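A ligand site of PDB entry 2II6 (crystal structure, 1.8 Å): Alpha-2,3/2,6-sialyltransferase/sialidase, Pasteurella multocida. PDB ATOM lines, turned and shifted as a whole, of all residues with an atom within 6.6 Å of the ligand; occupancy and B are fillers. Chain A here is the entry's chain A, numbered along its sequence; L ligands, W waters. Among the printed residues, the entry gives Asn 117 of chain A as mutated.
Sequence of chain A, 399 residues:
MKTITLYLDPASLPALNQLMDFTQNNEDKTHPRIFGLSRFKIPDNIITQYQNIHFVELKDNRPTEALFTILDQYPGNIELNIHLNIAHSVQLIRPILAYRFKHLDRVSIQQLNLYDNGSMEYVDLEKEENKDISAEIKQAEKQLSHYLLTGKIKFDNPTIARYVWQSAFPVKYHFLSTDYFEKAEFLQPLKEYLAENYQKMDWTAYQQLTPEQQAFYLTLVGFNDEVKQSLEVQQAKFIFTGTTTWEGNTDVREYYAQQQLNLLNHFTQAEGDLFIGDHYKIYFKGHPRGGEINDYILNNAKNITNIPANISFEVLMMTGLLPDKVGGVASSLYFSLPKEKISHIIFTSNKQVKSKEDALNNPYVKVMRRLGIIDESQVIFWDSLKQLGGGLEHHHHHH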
ATOM      1  N   SER A  12      10.917  28.050 -23.307  1.00  0.00           N
ATOM      2  CA  SER A  12      11.839  28.676 -24.257  1.00  0.00           C
ATOM      3  C   SER A  12      12.241  27.799 -25.450  1.00  0.00           C
ATOM      4  O   SER A  12      12.088  28.200 -26.621  1.00  0.00           O
ATOM      5  CB  SER A  12      13.065  29.201 -23.546  1.00  0.00           C
ATOM      6  OG  SER A  12      12.677  30.219 -22.633  1.00  0.00           O
ATOM      7  N   LEU A  13      12.732  26.589 -25.174  1.00  0.00           N
ATOM      8  CA  LEU A  13      13.289  25.775 -26.251  1.00  0.00           C
ATOM      9  C   LEU A  13      12.280  25.435 -27.343  1.00  0.00           C
ATOM     10  O   LEU A  13      12.580  25.632 -28.529  1.00  0.00           O
ATOM     11  CB  LEU A  13      14.065  24.556 -25.684  1.00  0.00           C
ATOM     12  CG  LEU A  13      14.733  23.621 -26.703  1.00  0.00           C
ATOM     13  CD1 LEU A  13      15.668  24.384 -27.668  1.00  0.00           C
ATOM     14  CD2 LEU A  13      15.499  22.508 -26.005  1.00  0.00           C
ATOM     15  N   ASN A 117      10.913  20.651 -23.797  1.00  0.00           N
ATOM     16  CA  ASN A 117      11.081  21.788 -22.874  1.00  0.00           C
ATOM     17  C   ASN A 117      12.573  21.918 -22.568  1.00  0.00           C
ATOM     18  O   ASN A 117      13.137  23.026 -22.616  1.00  0.00           O
ATOM     19  CB  ASN A 117      10.314  21.556 -21.592  1.00  0.00           C
ATOM     20  CG  ASN A 117      10.256  22.788 -20.689  1.00  0.00           C
ATOM     21  OD1 ASN A 117       9.237  23.477 -20.636  1.00  0.00           O
ATOM     22  ND2 ASN A 117      11.331  23.055 -19.953  1.00  0.00           N
ATOM     23  N   SER A 119      15.760  19.703 -20.106  1.00  0.00           N
ATOM     24  CA  SER A 119      16.098  18.602 -19.186  1.00  0.00           C
ATOM     25  C   SER A 119      14.850  18.052 -18.470  1.00  0.00           C
ATOM     26  O   SER A 119      14.826  16.910 -18.040  1.00  0.00           O
ATOM     27  CB  SER A 119      17.129  19.041 -18.138  1.00  0.00           C
ATOM     28  OG  SER A 119      16.626  20.124 -17.382  1.00  0.00           O
ATOM     29  N   PHE A 240      30.934  32.371 -19.387  1.00  0.00           N
ATOM     30  CA  PHE A 240      30.570  32.094 -17.987  1.00  0.00           C
ATOM     31  C   PHE A 240      29.054  32.219 -17.787  1.00  0.00           C
ATOM     32  O   PHE A 240      28.467  33.237 -18.137  1.00  0.00           O
ATOM     33  CB  PHE A 240      31.209  33.125 -17.075  1.00  0.00           C
ATOM     34  CG  PHE A 240      31.003  32.866 -15.609  1.00  0.00           C
ATOM     35  CD1 PHE A 240      31.915  32.072 -14.902  1.00  0.00           C
ATOM     36  CD2 PHE A 240      29.933  33.443 -14.909  1.00  0.00           C
ATOM     37  CE1 PHE A 240      31.755  31.840 -13.503  1.00  0.00           C
ATOM     38  CE2 PHE A 240      29.769  33.233 -13.512  1.00  0.00           C
ATOM     39  CZ  PHE A 240      30.686  32.420 -12.820  1.00  0.00           C
ATOM     40  N   THR A 241      28.461  31.231 -17.110  1.00  0.00           N
ATOM     41  CA  THR A 241      27.008  31.227 -16.916  1.00  0.00           C
ATOM     42  C   THR A 241      26.658  31.749 -15.522  1.00  0.00           C
ATOM     43  O   THR A 241      26.845  31.061 -14.526  1.00  0.00           O
ATOM     44  CB  THR A 241      26.458  29.833 -17.051  1.00  0.00           C
ATOM     45  OG1 THR A 241      27.163  28.950 -16.168  1.00  0.00           O
ATOM     46  CG2 THR A 241      26.587  29.351 -18.488  1.00  0.00           C
ATOM     47  N   GLY A 242      26.142  32.973 -15.455  1.00  0.00           N
ATOM     48  CA  GLY A 242      25.788  33.587 -14.179  1.00  0.00           C
ATOM     49  C   GLY A 242      24.493  33.021 -13.570  1.00  0.00           C
ATOM     50  O   GLY A 242      23.719  32.272 -14.216  1.00  0.00           O
ATOM     51  N   THR A 243      24.289  33.365 -12.302  1.00  0.00           N
ATOM     52  CA  THR A 243      23.099  32.967 -11.592  1.00  0.00           C
ATOM     53  C   THR A 243      22.450  34.176 -10.874  1.00  0.00           C
ATOM     54  O   THR A 243      22.863  35.314 -11.078  1.00  0.00           O
ATOM     55  CB  THR A 243      23.393  31.765 -10.619  1.00  0.00           C
ATOM     56  OG1 THR A 243      22.162  31.180 -10.174  1.00  0.00           O
ATOM     57  CG2 THR A 243      24.221  32.216  -9.393  1.00  0.00           C
ATOM     58  N   LYS A 285      27.432  35.525 -19.581  1.00  0.00           N
ATOM     59  CA  LYS A 285      26.018  35.299 -19.916  1.00  0.00           C
ATOM     60  C   LYS A 285      25.223  35.268 -18.621  1.00  0.00           C
ATOM     61  O   LYS A 285      25.128  34.211 -17.935  1.00  0.00           O
ATOM     62  CB  LYS A 285      25.868  34.023 -20.740  1.00  0.00           C
ATOM     63  CG  LYS A 285      24.470  33.573 -20.969  1.00  0.00           C
ATOM     64  CD  LYS A 285      23.683  34.511 -21.867  1.00  0.00           C
ATOM     65  CE  LYS A 285      22.596  35.215 -21.091  1.00  0.00           C
ATOM     66  NZ  LYS A 285      21.300  34.465 -20.819  1.00  0.00           N
ATOM     67  N   GLY A 286      24.707  36.428 -18.248  1.00  0.00           N
ATOM     68  CA  GLY A 286      23.933  36.561 -17.026  1.00  0.00           C
ATOM     69  C   GLY A 286      22.630  35.790 -17.077  1.00  0.00           C
ATOM     70  O   GLY A 286      22.086  35.519 -18.142  1.00  0.00           O
ATOM     71  N   HIS A 287      22.155  35.429 -15.892  1.00  0.00           N
ATOM     72  CA  HIS A 287      20.866  34.797 -15.726  1.00  0.00           C
ATOM     73  C   HIS A 287      19.793  35.817 -16.158  1.00  0.00           C
ATOM     74  O   HIS A 287      19.896  36.995 -15.847  1.00  0.00           O
ATOM     75  CB  HIS A 287      20.704  34.355 -14.250  1.00  0.00           C
ATOM     76  CG  HIS A 287      19.498  33.502 -13.989  1.00  0.00           C
ATOM     77  ND1 HIS A 287      18.210  33.979 -14.089  1.00  0.00           N
ATOM     78  CD2 HIS A 287      19.382  32.203 -13.604  1.00  0.00           C
ATOM     79  CE1 HIS A 287      17.349  33.015 -13.811  1.00  0.00           C
ATOM     80  NE2 HIS A 287      18.042  31.924 -13.523  1.00  0.00           N
ATOM     81  N   PRO A 288      18.749  35.369 -16.884  1.00  0.00           N
ATOM     82  CA  PRO A 288      17.697  36.321 -17.279  1.00  0.00           C
ATOM     83  C   PRO A 288      17.038  37.079 -16.128  1.00  0.00           C
ATOM     84  O   PRO A 288      16.526  38.162 -16.324  1.00  0.00           O
ATOM     85  CB  PRO A 288      16.665  35.441 -17.993  1.00  0.00           C
ATOM     86  CG  PRO A 288      16.944  34.079 -17.536  1.00  0.00           C
ATOM     87  CD  PRO A 288      18.454  34.029 -17.398  1.00  0.00           C
ATOM     88  N   ARG A 289      17.078  36.517 -14.921  1.00  0.00           N
ATOM     89  CA  ARG A 289      16.467  37.146 -13.761  1.00  0.00           C
ATOM     90  C   ARG A 289      17.499  37.747 -12.824  1.00  0.00           C
ATOM     91  O   ARG A 289      17.166  38.160 -11.714  1.00  0.00           O
ATOM     92  CB  ARG A 289      15.576  36.124 -13.030  1.00  0.00           C
ATOM     93  CG  ARG A 289      14.284  35.809 -13.778  1.00  0.00           C
ATOM     94  CD  ARG A 289      13.361  34.955 -12.936  1.00  0.00           C
ATOM     95  NE  ARG A 289      13.672  33.533 -13.095  1.00  0.00           N
ATOM     96  CZ  ARG A 289      14.345  32.779 -12.237  1.00  0.00           C
ATOM     97  NH1 ARG A 289      14.835  33.285 -11.097  1.00  0.00           N
ATOM     98  NH2 ARG A 289      14.544  31.494 -12.517  1.00  0.00           N
ATOM     99  N   ALA A 309      21.408  39.341 -21.001  1.00  0.00           N
ATOM    100  CA  ALA A 309      20.861  38.277 -20.121  1.00  0.00           C
ATOM    101  C   ALA A 309      19.511  37.739 -20.599  1.00  0.00           C
ATOM    102  O   ALA A 309      19.147  36.572 -20.336  1.00  0.00           O
ATOM    103  CB  ALA A 309      20.726  38.810 -18.675  1.00  0.00           C
ATOM    104  N   ASN A 310      18.784  38.599 -21.294  1.00  0.00           N
ATOM    105  CA  ASN A 310      17.413  38.342 -21.725  1.00  0.00           C
ATOM    106  C   ASN A 310      17.323  37.294 -22.837  1.00  0.00           C
ATOM    107  O   ASN A 310      16.242  36.720 -23.089  1.00  0.00           O
ATOM    108  CB  ASN A 310      16.787  39.671 -22.151  1.00  0.00           C
ATOM    109  CG  ASN A 310      17.796  40.617 -22.796  1.00  0.00           C
ATOM    110  OD1 ASN A 310      18.395  41.481 -22.127  1.00  0.00           O
ATOM    111  ND2 ASN A 310      18.038  40.398 -24.090  1.00  0.00           N
ATOM    112  N   ILE A 311      18.439  37.042 -23.512  1.00  0.00           N
ATOM    113  CA  ILE A 311      18.525  36.027 -24.565  1.00  0.00           C
ATOM    114  C   ILE A 311      18.592  34.643 -23.884  1.00  0.00           C
ATOM    115  O   ILE A 311      19.316  34.465 -22.888  1.00  0.00           O
ATOM    116  CB  ILE A 311      19.791  36.232 -25.470  1.00  0.00           C
ATOM    117  CG1 ILE A 311      19.820  37.655 -26.069  1.00  0.00           C
ATOM    118  CG2 ILE A 311      19.844  35.210 -26.604  1.00  0.00           C
ATOM    119  CD1 ILE A 311      21.201  38.084 -26.619  1.00  0.00           C
ATOM    120  N   SER A 312      17.792  33.686 -24.384  1.00  0.00           N
ATOM    121  CA  SER A 312      17.849  32.308 -23.868  1.00  0.00           C
ATOM    122  C   SER A 312      19.153  31.700 -24.352  1.00  0.00           C
ATOM    123  O   SER A 312      19.482  31.773 -25.552  1.00  0.00           O
ATOM    124  CB  SER A 312      16.679  31.457 -24.359  1.00  0.00           C
ATOM    125  OG  SER A 312      15.414  31.900 -23.850  1.00  0.00           O
ATOM    126  N   PHE A 313      19.874  31.062 -23.438  1.00  0.00           N
ATOM    127  CA  PHE A 313      21.155  30.420 -23.759  1.00  0.00           C
ATOM    128  C   PHE A 313      21.054  29.534 -25.011  1.00  0.00           C
ATOM    129  O   PHE A 313      21.977  29.516 -25.831  1.00  0.00           O
ATOM    130  CB  PHE A 313      21.738  29.635 -22.567  1.00  0.00           C
ATOM    131  CG  PHE A 313      23.211  29.296 -22.717  1.00  0.00           C
ATOM    132  CD1 PHE A 313      23.610  28.170 -23.444  1.00  0.00           C
ATOM    133  CD2 PHE A 313      24.192  30.117 -22.185  1.00  0.00           C
ATOM    134  CE1 PHE A 313      24.972  27.881 -23.637  1.00  0.00           C
ATOM    135  CE2 PHE A 313      25.555  29.833 -22.365  1.00  0.00           C
ATOM    136  CZ  PHE A 313      25.942  28.719 -23.096  1.00  0.00           C
ATOM    137  N   GLU A 314      19.939  28.817 -25.152  1.00  0.00           N
ATOM    138  CA  GLU A 314      19.761  27.845 -26.234  1.00  0.00           C
ATOM    139  C   GLU A 314      19.751  28.508 -27.625  1.00  0.00           C
ATOM    140  O   GLU A 314      19.882  27.818 -28.654  1.00  0.00           O
ATOM    141  CB  GLU A 314      18.478  27.027 -26.032  1.00  0.00           C
ATOM    142  CG  GLU A 314      18.522  26.057 -24.838  1.00  0.00           C
ATOM    143  CD  GLU A 314      18.311  26.734 -23.477  1.00  0.00           C
ATOM    144  OE1 GLU A 314      17.907  27.929 -23.447  1.00  0.00           O
ATOM    145  OE2 GLU A 314      18.587  26.066 -22.446  1.00  0.00           O
ATOM    146  N   VAL A 329      28.132  28.854 -13.055  1.00  0.00           N
ATOM    147  CA  VAL A 329      27.130  28.343 -12.107  1.00  0.00           C
ATOM    148  C   VAL A 329      26.163  27.455 -12.858  1.00  0.00           C
ATOM    149  O   VAL A 329      25.793  27.745 -13.982  1.00  0.00           O
ATOM    150  CB  VAL A 329      26.347  29.458 -11.390  1.00  0.00           C
ATOM    151  CG1 VAL A 329      25.317  28.847 -10.405  1.00  0.00           C
ATOM    152  CG2 VAL A 329      27.273  30.360 -10.629  1.00  0.00           C
ATOM    153  N   ALA A 330      25.795  26.349 -12.212  1.00  0.00           N
ATOM    154  CA  ALA A 330      24.924  25.340 -12.787  1.00  0.00           C
ATOM    155  C   ALA A 330      23.574  25.883 -13.217  1.00  0.00           C
ATOM    156  O   ALA A 330      23.035  26.774 -12.585  1.00  0.00           O
ATOM    157  CB  ALA A 330      24.719  24.210 -11.794  1.00  0.00           C
ATOM    158  N   SER A 331      23.073  25.298 -14.315  1.00  0.00           N
ATOM    159  CA  SER A 331      21.746  25.537 -14.889  1.00  0.00           C
ATOM    160  C   SER A 331      21.419  24.339 -15.751  1.00  0.00           C
ATOM    161  O   SER A 331      22.315  23.697 -16.255  1.00  0.00           O
ATOM    162  CB  SER A 331      21.773  26.772 -15.808  1.00  0.00           C
ATOM    163  OG  SER A 331      20.624  26.838 -16.659  1.00  0.00           O
ATOM    164  N   SER A 332      20.116  24.094 -15.949  1.00  0.00           N
ATOM    165  CA  SER A 332      19.663  23.021 -16.840  1.00  0.00           C
ATOM    166  C   SER A 332      20.137  23.183 -18.269  1.00  0.00           C
ATOM    167  O   SER A 332      20.057  22.244 -19.082  1.00  0.00           O
ATOM    168  CB  SER A 332      18.129  22.955 -16.825  1.00  0.00           C
ATOM    169  OG  SER A 332      17.552  24.132 -17.340  1.00  0.00           O
ATOM    170  N   LEU A 333      20.580  24.398 -18.610  1.00  0.00           N
ATOM    171  CA  LEU A 333      21.070  24.675 -19.951  1.00  0.00           C
ATOM    172  C   LEU A 333      22.261  23.737 -20.302  1.00  0.00           C
ATOM    173  O   LEU A 333      22.495  23.434 -21.465  1.00  0.00           O
ATOM    174  CB  LEU A 333      21.473  26.162 -20.079  1.00  0.00           C
ATOM    175  CG  LEU A 333      22.759  26.592 -19.350  1.00  0.00           C
ATOM    176  CD1 LEU A 333      24.005  26.259 -20.171  1.00  0.00           C
ATOM    177  CD2 LEU A 333      22.757  28.087 -18.930  1.00  0.00           C
ATOM    178  N   TYR A 364      19.398  16.151 -13.335  1.00  0.00           N
ATOM    179  CA  TYR A 364      19.919  16.239 -14.709  1.00  0.00           C
ATOM    180  C   TYR A 364      21.422  15.864 -14.752  1.00  0.00           C
ATOM    181  O   TYR A 364      21.883  15.230 -15.697  1.00  0.00           O
ATOM    182  CB  TYR A 364      19.618  17.605 -15.392  1.00  0.00           C
ATOM    183  CG  TYR A 364      20.266  18.847 -14.829  1.00  0.00           C
ATOM    184  CD1 TYR A 364      21.604  19.166 -15.120  1.00  0.00           C
ATOM    185  CD2 TYR A 364      19.540  19.749 -14.034  1.00  0.00           C
ATOM    186  CE1 TYR A 364      22.195  20.318 -14.609  1.00  0.00           C
ATOM    187  CE2 TYR A 364      20.131  20.901 -13.523  1.00  0.00           C
ATOM    188  CZ  TYR A 364      21.463  21.183 -13.828  1.00  0.00           C
ATOM    189  OH  TYR A 364      22.053  22.329 -13.330  1.00  0.00           O
HETATM  190  O1  LIG L   1      18.771  26.744 -14.590  1.00  0.00           O
HETATM  191  P1  LIG L   1      17.303  26.978 -15.120  1.00  0.00           P
HETATM  192  O2  LIG L   1      16.607  25.586 -15.469  1.00  0.00           O
HETATM  193  O3  LIG L   1      16.422  27.817 -14.093  1.00  0.00           O
HETATM  194  O4  LIG L   1      17.466  27.855 -16.449  1.00  0.00           O
HETATM  195  C1  LIG L   1      16.260  28.127 -17.142  1.00  0.00           C
HETATM  196  C2  LIG L   1      16.652  28.858 -18.411  1.00  0.00           C
HETATM  197  O5  LIG L   1      17.263  30.140 -18.198  1.00  0.00           O
HETATM  198  C3  LIG L   1      17.494  28.084 -19.413  1.00  0.00           C
HETATM  199  O6  LIG L   1      16.794  27.289 -20.374  1.00  0.00           O
HETATM  200  C4  LIG L   1      18.453  29.092 -19.992  1.00  0.00           C
HETATM  201  O7  LIG L   1      17.849  29.445 -21.239  1.00  0.00           O
HETATM  202  C5  LIG L   1      18.311  30.357 -19.156  1.00  0.00           C
HETATM  203  N1  LIG L   1      19.607  30.793 -18.585  1.00  0.00           N
HETATM  204  C6  LIG L   1      20.406  31.653 -19.373  1.00  0.00           C
HETATM  205  N2  LIG L   1      21.592  32.094 -18.895  1.00  0.00           N
HETATM  206  C7  LIG L   1      22.011  31.712 -17.653  1.00  0.00           C
HETATM  207  C8  LIG L   1      21.218  30.890 -16.852  1.00  0.00           C
HETATM  208  C9  LIG L   1      19.994  30.438 -17.348  1.00  0.00           C
HETATM  209  O8  LIG L   1      20.044  31.976 -20.544  1.00  0.00           O
HETATM  210  N3  LIG L   1      23.201  32.164 -17.196  1.00  0.00           N
HETATM  211  O   HOH W   1      19.895  27.235 -12.485  1.00  0.00           O
HETATM  212  O   HOH W   2      15.269  31.070 -21.313  1.00  0.00           O
HETATM  213  O   HOH W   3      14.274  25.212 -17.967  1.00  0.00           O
HETATM  214  O   HOH W   4      14.079  26.876 -20.501  1.00  0.00           O
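The side-chain hydroxyl (OG) of Ser 332 sits at hydrogen-bond distance from an oxygen (O2) of the ligand, 2.6 Å away. The backbone carbonyl oxygen (O) of Lys 285 is in hydrogen-bond range of a nitrogen (N3) of the ligand. O1 of the ligand sits at hydrogen-bond distance from OG of Ser 331, 2.8 Å away. The backbone carbonyl oxygen (O) of Gly 242 sits at hydrogen-bond distance from a nitrogen (N3) of the ligand, 3.0 Å away. O1 of the ligand lies within hydrogen-bond range of N of Ser 332 (3.3 Å). The backbone NH (N) of Phe 313 sits at hydrogen-bond distance from an oxygen (O8) of the ligand (3.0 Å). The side-chain carboxylate (OE1) of Glu 314 is in hydrogen-bond range of an oxygen (O7) of the ligand, at 2.7 Å. NZ of Lys 285 is in hydrogen-bond range of O8 of the ligand (2.8 Å).
Water W1 lies within hydrogen-bond range of O1 of the ligand (2.4 Å) and O of Ala 330 (3.2 Å). Water W2 lies within hydrogen-bond range of OG of Ser 312, OG of Ser 12 and O7 of the ligand.
NZ of Lys 285 sits at hydrogen-bond distance from O of Ala 309 (3.1 Å). OG of Ser 331 sits close to N of Leu 333 (3.1 Å). ND1 of His 287 is in hydrogen-bond range of N of Arg 289 (2.9 Å). N of Lys 285 sits at hydrogen-bond distance from O of Phe 240, 2.9 Å away. NZ of Lys 285 lies within hydrogen-bond range of O of Ile 311, 2.9 Å away. The side-chain hydroxyl of Tyr 364 sits close to the backbone carbonyl oxygen of Ser 331 (3.2 Å). The side-chain hydroxyl (OG) of Ser 12 sits at hydrogen-bond distance from the side-chain hydroxyl (OG) of Ser 312 (3.4 Å). OG1 of Thr 241 is in hydrogen-bond range of O of Val 329, at 2.8 Å.
O of Ile 311 lies close to O8 of the ligand, at 3.5 Å. C of Thr 241 touches N3 of the ligand, 3.9 Å away. Gly 286 touches the ligand. His 287 touches the ligand. CD of Pro 288 touches N1 of the ligand, 3.6 Å away. Ser 312 touches the ligand. Leu 333 touches the ligand (CD2 to C8, 3.8 Å). 13 residues have an atom within 4 Å of the ligand: Thr 241, Gly 242, Lys 285, Gly 286, His 287, Pro 288, Ile 311, Ser 312, Phe 313, Glu 314, Ser 331, Ser 332 and Leu 333.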
